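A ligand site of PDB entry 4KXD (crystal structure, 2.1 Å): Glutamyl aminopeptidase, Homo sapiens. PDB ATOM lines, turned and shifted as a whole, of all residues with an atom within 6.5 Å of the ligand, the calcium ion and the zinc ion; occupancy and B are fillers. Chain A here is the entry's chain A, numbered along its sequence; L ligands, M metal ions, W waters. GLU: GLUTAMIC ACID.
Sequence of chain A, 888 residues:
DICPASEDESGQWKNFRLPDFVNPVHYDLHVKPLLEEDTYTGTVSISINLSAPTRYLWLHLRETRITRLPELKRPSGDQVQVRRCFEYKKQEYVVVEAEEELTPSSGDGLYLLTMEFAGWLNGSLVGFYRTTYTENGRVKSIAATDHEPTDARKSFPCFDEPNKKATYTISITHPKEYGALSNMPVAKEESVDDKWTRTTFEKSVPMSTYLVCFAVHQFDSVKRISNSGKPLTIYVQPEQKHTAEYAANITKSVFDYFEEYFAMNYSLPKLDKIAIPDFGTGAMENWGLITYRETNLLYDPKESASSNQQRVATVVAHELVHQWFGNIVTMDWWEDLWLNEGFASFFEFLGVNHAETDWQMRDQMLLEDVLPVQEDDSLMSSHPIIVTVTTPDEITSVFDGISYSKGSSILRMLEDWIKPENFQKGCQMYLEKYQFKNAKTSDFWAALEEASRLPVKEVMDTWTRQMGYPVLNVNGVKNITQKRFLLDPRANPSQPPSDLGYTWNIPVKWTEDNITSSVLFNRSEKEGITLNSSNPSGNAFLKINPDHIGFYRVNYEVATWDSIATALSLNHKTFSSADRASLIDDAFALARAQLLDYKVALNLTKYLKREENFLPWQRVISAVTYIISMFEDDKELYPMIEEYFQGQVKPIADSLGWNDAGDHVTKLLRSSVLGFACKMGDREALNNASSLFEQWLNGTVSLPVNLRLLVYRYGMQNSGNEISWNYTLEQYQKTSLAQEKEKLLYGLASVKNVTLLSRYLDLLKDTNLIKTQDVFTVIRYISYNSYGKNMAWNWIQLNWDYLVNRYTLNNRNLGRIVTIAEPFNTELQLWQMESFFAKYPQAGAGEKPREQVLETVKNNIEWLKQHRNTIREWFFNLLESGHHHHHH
Merely in contact with the ligand: Met 284 and Phe 399.
Of the 25 residues printed, 11 come within 4 Å of the ligand.
The nearest printed residue that does not touch the ligand is His 322 (4.2 Å).
The zinc ion is bound by OE1 of Glu 341 (2.0 Å), NE2 of His 322 (2.2 Å) and NE2 of His 318 (2.3 Å).
The zinc ion has three donor atoms within binding distance.
The calcium ion is bound by the backbone carbonyl oxygen (O) of Glu 148 (2.3 Å).
Water W3 is bound to the calcium ion, 2.3 Å away.
The calcium ion is bound by OD2 of Asp 146, at 2.4 Å.
Water W1 is bound to the calcium ion.
The calcium ion is bound by water W4.
OE2 of the ligand is bound to the calcium ion.
Tyr 404 touches the zinc ion.
Within 4 Å of the zinc ion: His 318, His 322, Glu 341 and Tyr 404.
The side-chain hydroxyl (OH) of Tyr 404 lies close to the side-chain carboxylate (OE2) of Glu 341.
The backbone carbonyl oxygen of Glu 341 lies within hydrogen-bond range of the side-chain hydroxyl of Ser 345 (2.7 Å).
The guanidinium group (NH2) of Arg 812 lies within hydrogen-bond range of the side-chain hydroxyl (OG1) of Thr 396, 2.6 Å away.
O of Tyr 404 lies close to OG of Ser 345 (3.5 Å).
The side-chain carboxylate (OE1) of Glu 319 lies within hydrogen-bond range of the backbone NH (N) of Glu 285 (3.2 Å).
The side-chain carboxylate (OE2) of Glu 341 is in salt-bridge range of a nitrogen (N) of the ligand, 3.2 Å away.
OE1 of Glu 148 lies within salt-bridge range of N of the ligand, 3.4 Å away.
An oxygen (OE1) of the ligand is in salt-bridge range of the guanidinium group (NH1) of Arg 812 (2.5 Å).
The side-chain hydroxyl (OH) of Tyr 404 is in hydrogen-bond range of an oxygen (OXT) of the ligand, 2.6 Å away.
The side-chain carboxylate (OE2) of Glu 319 sits close to an oxygen (O) of the ligand (2.7 Å).
O of the ligand lies close to O of Ala 283.
OE1 of Glu 285 lies within salt-bridge range of N of the ligand, at 3.0 Å.
The side-chain hydroxyl (OG1) of Thr 281 lies close to an oxygen (OE2) of the ligand (3.4 Å).
Two residues have an atom within 4 Å of the calcium ion: Asp 146 and Glu 148.
The nearest printed residue that does not touch the calcium ion is His 147 (4.03 Å).
Water W1 lies within hydrogen-bond range of OD2 of Asp 151 (2.6 Å), O of Asp 146 (2.9 Å) and N of His 147 (3.5 Å).
Water W3 lies within hydrogen-bond range of the side-chain carboxylate of Asp 146 (2.7 Å), the backbone NH of Glu 148 (3.0 Å) and the side-chain sulfur of Met 284 (3.2 Å).
Water W2 lies within hydrogen-bond range of an oxygen (O) of the ligand (2.7 Å), the backbone NH of Gly 282 (3.3 Å) and the backbone NH of Ala 283 (3.3 Å).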
ATOM      1  N   LEU A 125      34.680  23.234  -0.871  1.00  0.00           N
ATOM      2  CA  LEU A 125      34.723  23.031   0.582  1.00  0.00           C
ATOM      3  C   LEU A 125      33.687  22.004   1.053  1.00  0.00           C
ATOM      4  O   LEU A 125      33.488  21.815   2.255  1.00  0.00           O
ATOM      5  CB  LEU A 125      34.560  24.385   1.303  1.00  0.00           C
ATOM      6  CG  LEU A 125      35.775  25.061   1.964  1.00  0.00           C
ATOM      7  CD1 LEU A 125      37.084  24.869   1.225  1.00  0.00           C
ATOM      8  CD2 LEU A 125      35.529  26.548   2.223  1.00  0.00           C
ATOM      9  N   VAL A 126      33.037  21.327   0.108  1.00  0.00           N
ATOM     10  CA  VAL A 126      32.038  20.295   0.454  1.00  0.00           C
ATOM     11  C   VAL A 126      32.441  18.947  -0.131  1.00  0.00           C
ATOM     12  O   VAL A 126      33.301  18.888  -1.012  1.00  0.00           O
ATOM     13  CB  VAL A 126      30.607  20.679   0.000  1.00  0.00           C
ATOM     14  CG1 VAL A 126      30.152  21.970   0.692  1.00  0.00           C
ATOM     15  CG2 VAL A 126      30.535  20.843  -1.507  1.00  0.00           C
ATOM     16  N   ASP A 146      32.932  17.343   4.423  1.00  0.00           N
ATOM     17  CA  ASP A 146      31.831  18.092   4.987  1.00  0.00           C
ATOM     18  C   ASP A 146      30.563  17.846   4.181  1.00  0.00           C
ATOM     19  O   ASP A 146      30.523  18.094   2.977  1.00  0.00           O
ATOM     20  CB  ASP A 146      32.138  19.590   5.031  1.00  0.00           C
ATOM     21  CG  ASP A 146      31.127  20.350   5.854  1.00  0.00           C
ATOM     22  OD1 ASP A 146      31.037  20.100   7.073  1.00  0.00           O
ATOM     23  OD2 ASP A 146      30.387  21.169   5.270  1.00  0.00           O
ATOM     24  N   HIS A 147      29.506  17.387   4.856  1.00  0.00           N
ATOM     25  CA  HIS A 147      28.348  16.834   4.153  1.00  0.00           C
ATOM     26  C   HIS A 147      26.984  17.518   4.330  1.00  0.00           C
ATOM     27  O   HIS A 147      26.164  17.438   3.419  1.00  0.00           O
ATOM     28  CB  HIS A 147      28.222  15.362   4.502  1.00  0.00           C
ATOM     29  CG  HIS A 147      29.368  14.526   4.016  1.00  0.00           C
ATOM     30  ND1 HIS A 147      29.805  13.401   4.701  1.00  0.00           N
ATOM     31  CD2 HIS A 147      30.176  14.648   2.943  1.00  0.00           C
ATOM     32  CE1 HIS A 147      30.830  12.872   4.059  1.00  0.00           C
ATOM     33  NE2 HIS A 147      31.072  13.608   2.979  1.00  0.00           N
ATOM     34  N   GLU A 148      26.717  18.163   5.457  1.00  0.00           N
ATOM     35  CA  GLU A 148      25.361  18.667   5.732  1.00  0.00           C
ATOM     36  C   GLU A 148      25.011  19.882   4.885  1.00  0.00           C
ATOM     37  O   GLU A 148      25.777  20.851   4.832  1.00  0.00           O
ATOM     38  CB  GLU A 148      25.143  18.948   7.224  1.00  0.00           C
ATOM     39  CG  GLU A 148      23.682  19.018   7.676  1.00  0.00           C
ATOM     40  CD  GLU A 148      23.526  19.221   9.183  1.00  0.00           C
ATOM     41  OE1 GLU A 148      24.470  19.745   9.820  1.00  0.00           O
ATOM     42  OE2 GLU A 148      22.461  18.880   9.725  1.00  0.00           O
ATOM     43  N   PRO A 149      23.847  19.841   4.208  1.00  0.00           N
ATOM     44  CA  PRO A 149      22.886  18.738   4.260  1.00  0.00           C
ATOM     45  C   PRO A 149      22.963  17.672   3.172  1.00  0.00           C
ATOM     46  O   PRO A 149      22.724  16.514   3.458  1.00  0.00           O
ATOM     47  CB  PRO A 149      21.549  19.456   4.167  1.00  0.00           C
ATOM     48  CG  PRO A 149      21.843  20.639   3.301  1.00  0.00           C
ATOM     49  CD  PRO A 149      23.236  21.075   3.670  1.00  0.00           C
ATOM     50  N   ASP A 151      25.594  16.851   0.768  1.00  0.00           N
ATOM     51  CA  ASP A 151      26.907  16.725   0.128  1.00  0.00           C
ATOM     52  C   ASP A 151      27.651  15.391   0.361  1.00  0.00           C
ATOM     53  O   ASP A 151      28.720  15.151  -0.212  1.00  0.00           O
ATOM     54  CB  ASP A 151      27.808  17.921   0.489  1.00  0.00           C
ATOM     55  CG  ASP A 151      27.275  19.252  -0.050  1.00  0.00           C
ATOM     56  OD1 ASP A 151      26.907  19.327  -1.240  1.00  0.00           O
ATOM     57  OD2 ASP A 151      27.245  20.228   0.723  1.00  0.00           O
ATOM     58  N   GLY A 280      34.052  25.448   5.304  1.00  0.00           N
ATOM     59  CA  GLY A 280      32.888  26.139   4.741  1.00  0.00           C
ATOM     60  C   GLY A 280      31.760  26.616   5.631  1.00  0.00           C
ATOM     61  O   GLY A 280      30.973  27.468   5.201  1.00  0.00           O
ATOM     62  N   THR A 281      31.644  26.073   6.842  1.00  0.00           N
ATOM     63  CA  THR A 281      30.672  26.566   7.839  1.00  0.00           C
ATOM     64  C   THR A 281      31.350  26.871   9.171  1.00  0.00           C
ATOM     65  O   THR A 281      32.575  26.942   9.262  1.00  0.00           O
ATOM     66  CB  THR A 281      29.457  25.631   8.097  1.00  0.00           C
ATOM     67  OG1 THR A 281      29.848  24.249   8.008  1.00  0.00           O
ATOM     68  CG2 THR A 281      28.400  25.918   7.116  1.00  0.00           C
ATOM     69  N   GLY A 282      30.548  27.062  10.206  1.00  0.00           N
ATOM     70  CA  GLY A 282      31.086  27.356  11.512  1.00  0.00           C
ATOM     71  C   GLY A 282      31.709  26.106  12.109  1.00  0.00           C
ATOM     72  O   GLY A 282      32.830  26.120  12.592  1.00  0.00           O
ATOM     73  N   ALA A 283      30.935  25.035  12.063  1.00  0.00           N
ATOM     74  CA  ALA A 283      31.325  23.734  12.588  1.00  0.00           C
ATOM     75  C   ALA A 283      30.293  22.695  12.191  1.00  0.00           C
ATOM     76  O   ALA A 283      29.191  23.040  11.763  1.00  0.00           O
ATOM     77  CB  ALA A 283      31.464  23.796  14.100  1.00  0.00           C
ATOM     78  N   MET A 284      30.661  21.426  12.321  1.00  0.00           N
ATOM     79  CA  MET A 284      29.818  20.320  11.947  1.00  0.00           C
ATOM     80  C   MET A 284      29.935  19.202  12.983  1.00  0.00           C
ATOM     81  O   MET A 284      31.038  18.858  13.411  1.00  0.00           O
ATOM     82  CB  MET A 284      30.182  19.834  10.543  1.00  0.00           C
ATOM     83  CG  MET A 284      29.277  18.748   9.991  1.00  0.00           C
ATOM     84  SD  MET A 284      27.529  19.165  10.028  1.00  0.00           S
ATOM     85  CE  MET A 284      26.815  17.557   9.705  1.00  0.00           C
ATOM     86  N   GLU A 285      28.796  18.650  13.392  1.00  0.00           N
ATOM     87  CA  GLU A 285      28.714  17.742  14.516  1.00  0.00           C
ATOM     88  C   GLU A 285      28.978  16.281  14.153  1.00  0.00           C
ATOM     89  O   GLU A 285      28.481  15.373  14.842  1.00  0.00           O
ATOM     90  CB  GLU A 285      27.327  17.818  15.145  1.00  0.00           C
ATOM     91  CG  GLU A 285      26.206  17.452  14.185  1.00  0.00           C
ATOM     92  CD  GLU A 285      25.616  18.652  13.457  1.00  0.00           C
ATOM     93  OE1 GLU A 285      26.184  19.773  13.538  1.00  0.00           O
ATOM     94  OE2 GLU A 285      24.576  18.465  12.798  1.00  0.00           O
ATOM     95  N   VAL A 315      30.064  27.379  20.578  1.00  0.00           N
ATOM     96  CA  VAL A 315      30.090  26.498  19.395  1.00  0.00           C
ATOM     97  C   VAL A 315      30.451  25.080  19.836  1.00  0.00           C
ATOM     98  O   VAL A 315      29.812  24.113  19.423  1.00  0.00           O
ATOM     99  CB  VAL A 315      31.000  26.996  18.260  1.00  0.00           C
ATOM    100  CG1 VAL A 315      30.961  26.044  17.079  1.00  0.00           C
ATOM    101  CG2 VAL A 315      30.559  28.366  17.785  1.00  0.00           C
ATOM    102  N   HIS A 318      27.431  23.790  21.517  1.00  0.00           N
ATOM    103  CA  HIS A 318      26.476  23.577  20.424  1.00  0.00           C
ATOM    104  C   HIS A 318      26.698  22.224  19.782  1.00  0.00           C
ATOM    105  O   HIS A 318      25.765  21.426  19.670  1.00  0.00           O
ATOM    106  CB  HIS A 318      26.602  24.682  19.379  1.00  0.00           C
ATOM    107  CG  HIS A 318      25.562  24.634  18.299  1.00  0.00           C
ATOM    108  ND1 HIS A 318      24.405  25.396  18.350  1.00  0.00           N
ATOM    109  CD2 HIS A 318      25.494  23.921  17.157  1.00  0.00           C
ATOM    110  CE1 HIS A 318      23.679  25.151  17.270  1.00  0.00           C
ATOM    111  NE2 HIS A 318      24.318  24.260  16.534  1.00  0.00           N
ATOM    112  N   GLU A 319      27.937  21.969  19.363  1.00  0.00           N
ATOM    113  CA  GLU A 319      28.281  20.739  18.654  1.00  0.00           C
ATOM    114  C   GLU A 319      28.130  19.527  19.552  1.00  0.00           C
ATOM    115  O   GLU A 319      27.758  18.466  19.090  1.00  0.00           O
ATOM    116  CB  GLU A 319      29.703  20.818  18.074  1.00  0.00           C
ATOM    117  CG  GLU A 319      29.940  21.922  17.064  1.00  0.00           C
ATOM    118  CD  GLU A 319      28.857  22.035  16.029  1.00  0.00           C
ATOM    119  OE1 GLU A 319      28.445  21.004  15.466  1.00  0.00           O
ATOM    120  OE2 GLU A 319      28.387  23.153  15.764  1.00  0.00           O
ATOM    121  N   HIS A 322      24.486  18.247  19.779  1.00  0.00           N
ATOM    122  CA  HIS A 322      24.166  17.412  18.627  1.00  0.00           C
ATOM    123  C   HIS A 322      24.518  15.945  18.808  1.00  0.00           C
ATOM    124  O   HIS A 322      23.891  15.081  18.181  1.00  0.00           O
ATOM    125  CB  HIS A 322      24.847  17.937  17.363  1.00  0.00           C
ATOM    126  CG  HIS A 322      24.155  19.104  16.733  1.00  0.00           C
ATOM    127  ND1 HIS A 322      22.822  19.070  16.364  1.00  0.00           N
ATOM    128  CD2 HIS A 322      24.616  20.316  16.356  1.00  0.00           C
ATOM    129  CE1 HIS A 322      22.502  20.229  15.808  1.00  0.00           C
ATOM    130  NE2 HIS A 322      23.566  21.000  15.789  1.00  0.00           N
ATOM    131  N   ASN A 340      16.979  19.483  15.399  1.00  0.00           N
ATOM    132  CA  ASN A 340      18.431  19.445  15.526  1.00  0.00           C
ATOM    133  C   ASN A 340      18.944  20.790  16.009  1.00  0.00           C
ATOM    134  O   ASN A 340      19.531  20.897  17.086  1.00  0.00           O
ATOM    135  CB  ASN A 340      19.078  19.111  14.180  1.00  0.00           C
ATOM    136  CG  ASN A 340      19.113  17.616  13.879  1.00  0.00           C
ATOM    137  OD1 ASN A 340      20.002  17.153  13.172  1.00  0.00           O
ATOM    138  ND2 ASN A 340      18.159  16.861  14.414  1.00  0.00           N
ATOM    139  N   GLU A 341      18.706  21.817  15.203  1.00  0.00           N
ATOM    140  CA  GLU A 341      19.364  23.096  15.353  1.00  0.00           C
ATOM    141  C   GLU A 341      18.838  23.959  16.495  1.00  0.00           C
ATOM    142  O   GLU A 341      19.618  24.638  17.181  1.00  0.00           O
ATOM    143  CB  GLU A 341      19.347  23.870  14.038  1.00  0.00           C
ATOM    144  CG  GLU A 341      19.995  23.107  12.881  1.00  0.00           C
ATOM    145  CD  GLU A 341      21.444  22.753  13.121  1.00  0.00           C
ATOM    146  OE1 GLU A 341      22.031  23.199  14.119  1.00  0.00           O
ATOM    147  OE2 GLU A 341      22.020  22.012  12.301  1.00  0.00           O
ATOM    148  N   ALA A 344      20.117  22.353  19.766  1.00  0.00           N
ATOM    149  CA  ALA A 344      21.512  22.732  19.938  1.00  0.00           C
ATOM    150  C   ALA A 344      21.643  24.208  20.330  1.00  0.00           C
ATOM    151  O   ALA A 344      22.386  24.543  21.250  1.00  0.00           O
ATOM    152  CB  ALA A 344      22.307  22.418  18.694  1.00  0.00           C
ATOM    153  N   SER A 345      20.885  25.070  19.648  1.00  0.00           N
ATOM    154  CA  SER A 345      20.898  26.504  19.940  1.00  0.00           C
ATOM    155  C   SER A 345      20.341  26.824  21.337  1.00  0.00           C
ATOM    156  O   SER A 345      20.717  27.840  21.932  1.00  0.00           O
ATOM    157  CB  SER A 345      20.110  27.308  18.885  1.00  0.00           C
ATOM    158  OG  SER A 345      20.629  27.112  17.585  1.00  0.00           O
ATOM    159  N   THR A 396      18.969  23.507   2.110  1.00  0.00           N
ATOM    160  CA  THR A 396      20.085  24.216   2.724  1.00  0.00           C
ATOM    161  C   THR A 396      19.721  25.629   3.173  1.00  0.00           C
ATOM    162  O   THR A 396      20.327  26.163   4.103  1.00  0.00           O
ATOM    163  CB  THR A 396      21.332  24.233   1.821  1.00  0.00           C
ATOM    164  OG1 THR A 396      22.473  24.571   2.614  1.00  0.00           O
ATOM    165  CG2 THR A 396      21.202  25.227   0.679  1.00  0.00           C
ATOM    166  N   PHE A 399      18.687  26.351   7.025  1.00  0.00           N
ATOM    167  CA  PHE A 399      19.693  26.495   8.069  1.00  0.00           C
ATOM    168  C   PHE A 399      19.808  27.998   8.350  1.00  0.00           C
ATOM    169  O   PHE A 399      20.723  28.659   7.871  1.00  0.00           O
ATOM    170  CB  PHE A 399      21.031  25.912   7.608  1.00  0.00           C
ATOM    171  CG  PHE A 399      21.058  24.394   7.595  1.00  0.00           C
ATOM    172  CD1 PHE A 399      20.553  23.684   6.514  1.00  0.00           C
ATOM    173  CD2 PHE A 399      21.596  23.686   8.664  1.00  0.00           C
ATOM    174  CE1 PHE A 399      20.569  22.297   6.508  1.00  0.00           C
ATOM    175  CE2 PHE A 399      21.626  22.300   8.659  1.00  0.00           C
ATOM    176  CZ  PHE A 399      21.105  21.605   7.588  1.00  0.00           C
ATOM    177  N   TYR A 404      17.382  27.967  13.995  1.00  0.00           N
ATOM    178  CA  TYR A 404      18.296  28.136  15.126  1.00  0.00           C
ATOM    179  C   TYR A 404      17.712  29.027  16.236  1.00  0.00           C
ATOM    180  O   TYR A 404      17.502  28.572  17.360  1.00  0.00           O
ATOM    181  CB  TYR A 404      19.635  28.728  14.660  1.00  0.00           C
ATOM    182  CG  TYR A 404      20.537  27.776  13.881  1.00  0.00           C
ATOM    183  CD1 TYR A 404      20.266  27.449  12.545  1.00  0.00           C
ATOM    184  CD2 TYR A 404      21.674  27.237  14.467  1.00  0.00           C
ATOM    185  CE1 TYR A 404      21.100  26.597  11.838  1.00  0.00           C
ATOM    186  CE2 TYR A 404      22.514  26.382  13.766  1.00  0.00           C
ATOM    187  CZ  TYR A 404      22.228  26.062  12.452  1.00  0.00           C
ATOM    188  OH  TYR A 404      23.053  25.214  11.756  1.00  0.00           O
ATOM    189  N   ARG A 812      24.943  28.303   0.648  1.00  0.00           N
ATOM    190  CA  ARG A 812      24.102  29.138   1.499  1.00  0.00           C
ATOM    191  C   ARG A 812      24.678  30.542   1.668  1.00  0.00           C
ATOM    192  O   ARG A 812      23.950  31.505   1.543  1.00  0.00           O
ATOM    193  CB  ARG A 812      23.970  28.426   2.840  1.00  0.00           C
ATOM    194  CG  ARG A 812      23.032  28.987   3.886  1.00  0.00           C
ATOM    195  CD  ARG A 812      23.137  28.142   5.143  1.00  0.00           C
ATOM    196  NE  ARG A 812      23.090  26.718   4.814  1.00  0.00           N
ATOM    197  CZ  ARG A 812      23.879  25.767   5.330  1.00  0.00           C
ATOM    198  NH1 ARG A 812      24.805  26.039   6.231  1.00  0.00           N
ATOM    199  NH2 ARG A 812      23.731  24.511   4.921  1.00  0.00           N
HETATM  200  N   GLU L   1      25.170  22.148  12.073  1.00  0.00           N
HETATM  201  CA  GLU L   1      26.265  23.131  11.849  1.00  0.00           C
HETATM  202  C   GLU L   1      26.287  24.253  12.874  1.00  0.00           C
HETATM  203  O   GLU L   1      27.232  24.380  13.654  1.00  0.00           O
HETATM  204  CB  GLU L   1      26.197  23.728  10.443  1.00  0.00           C
HETATM  205  CG  GLU L   1      26.531  22.760   9.329  1.00  0.00           C
HETATM  206  CD  GLU L   1      26.200  23.317   7.954  1.00  0.00           C
HETATM  207  OE1 GLU L   1      25.283  24.143   7.834  1.00  0.00           O
HETATM  208  OE2 GLU L   1      26.872  22.936   6.974  1.00  0.00           O
HETATM  209  OXT GLU L   1      25.372  25.070  12.957  1.00  0.00           O
HETATM  210 CA    CA M   1      28.012  21.344   5.072  1.00  0.00          CA
HETATM  211 ZN    ZN M   2      23.862  22.899  14.781  1.00  0.00          ZN
HETATM  212  O   HOH W   1      28.409  20.112   3.024  1.00  0.00           O
HETATM  213  O   HOH W   2      28.010  26.587  12.261  1.00  0.00           O
HETATM  214  O   HOH W   3      28.294  20.210   7.061  1.00  0.00           O
HETATM  215  O   HOH W   4      27.758  23.909   4.441  1.00  0.00           O
HETATM  216  O   HOH W   5      26.483  26.985  15.290  1.00  0.00           O
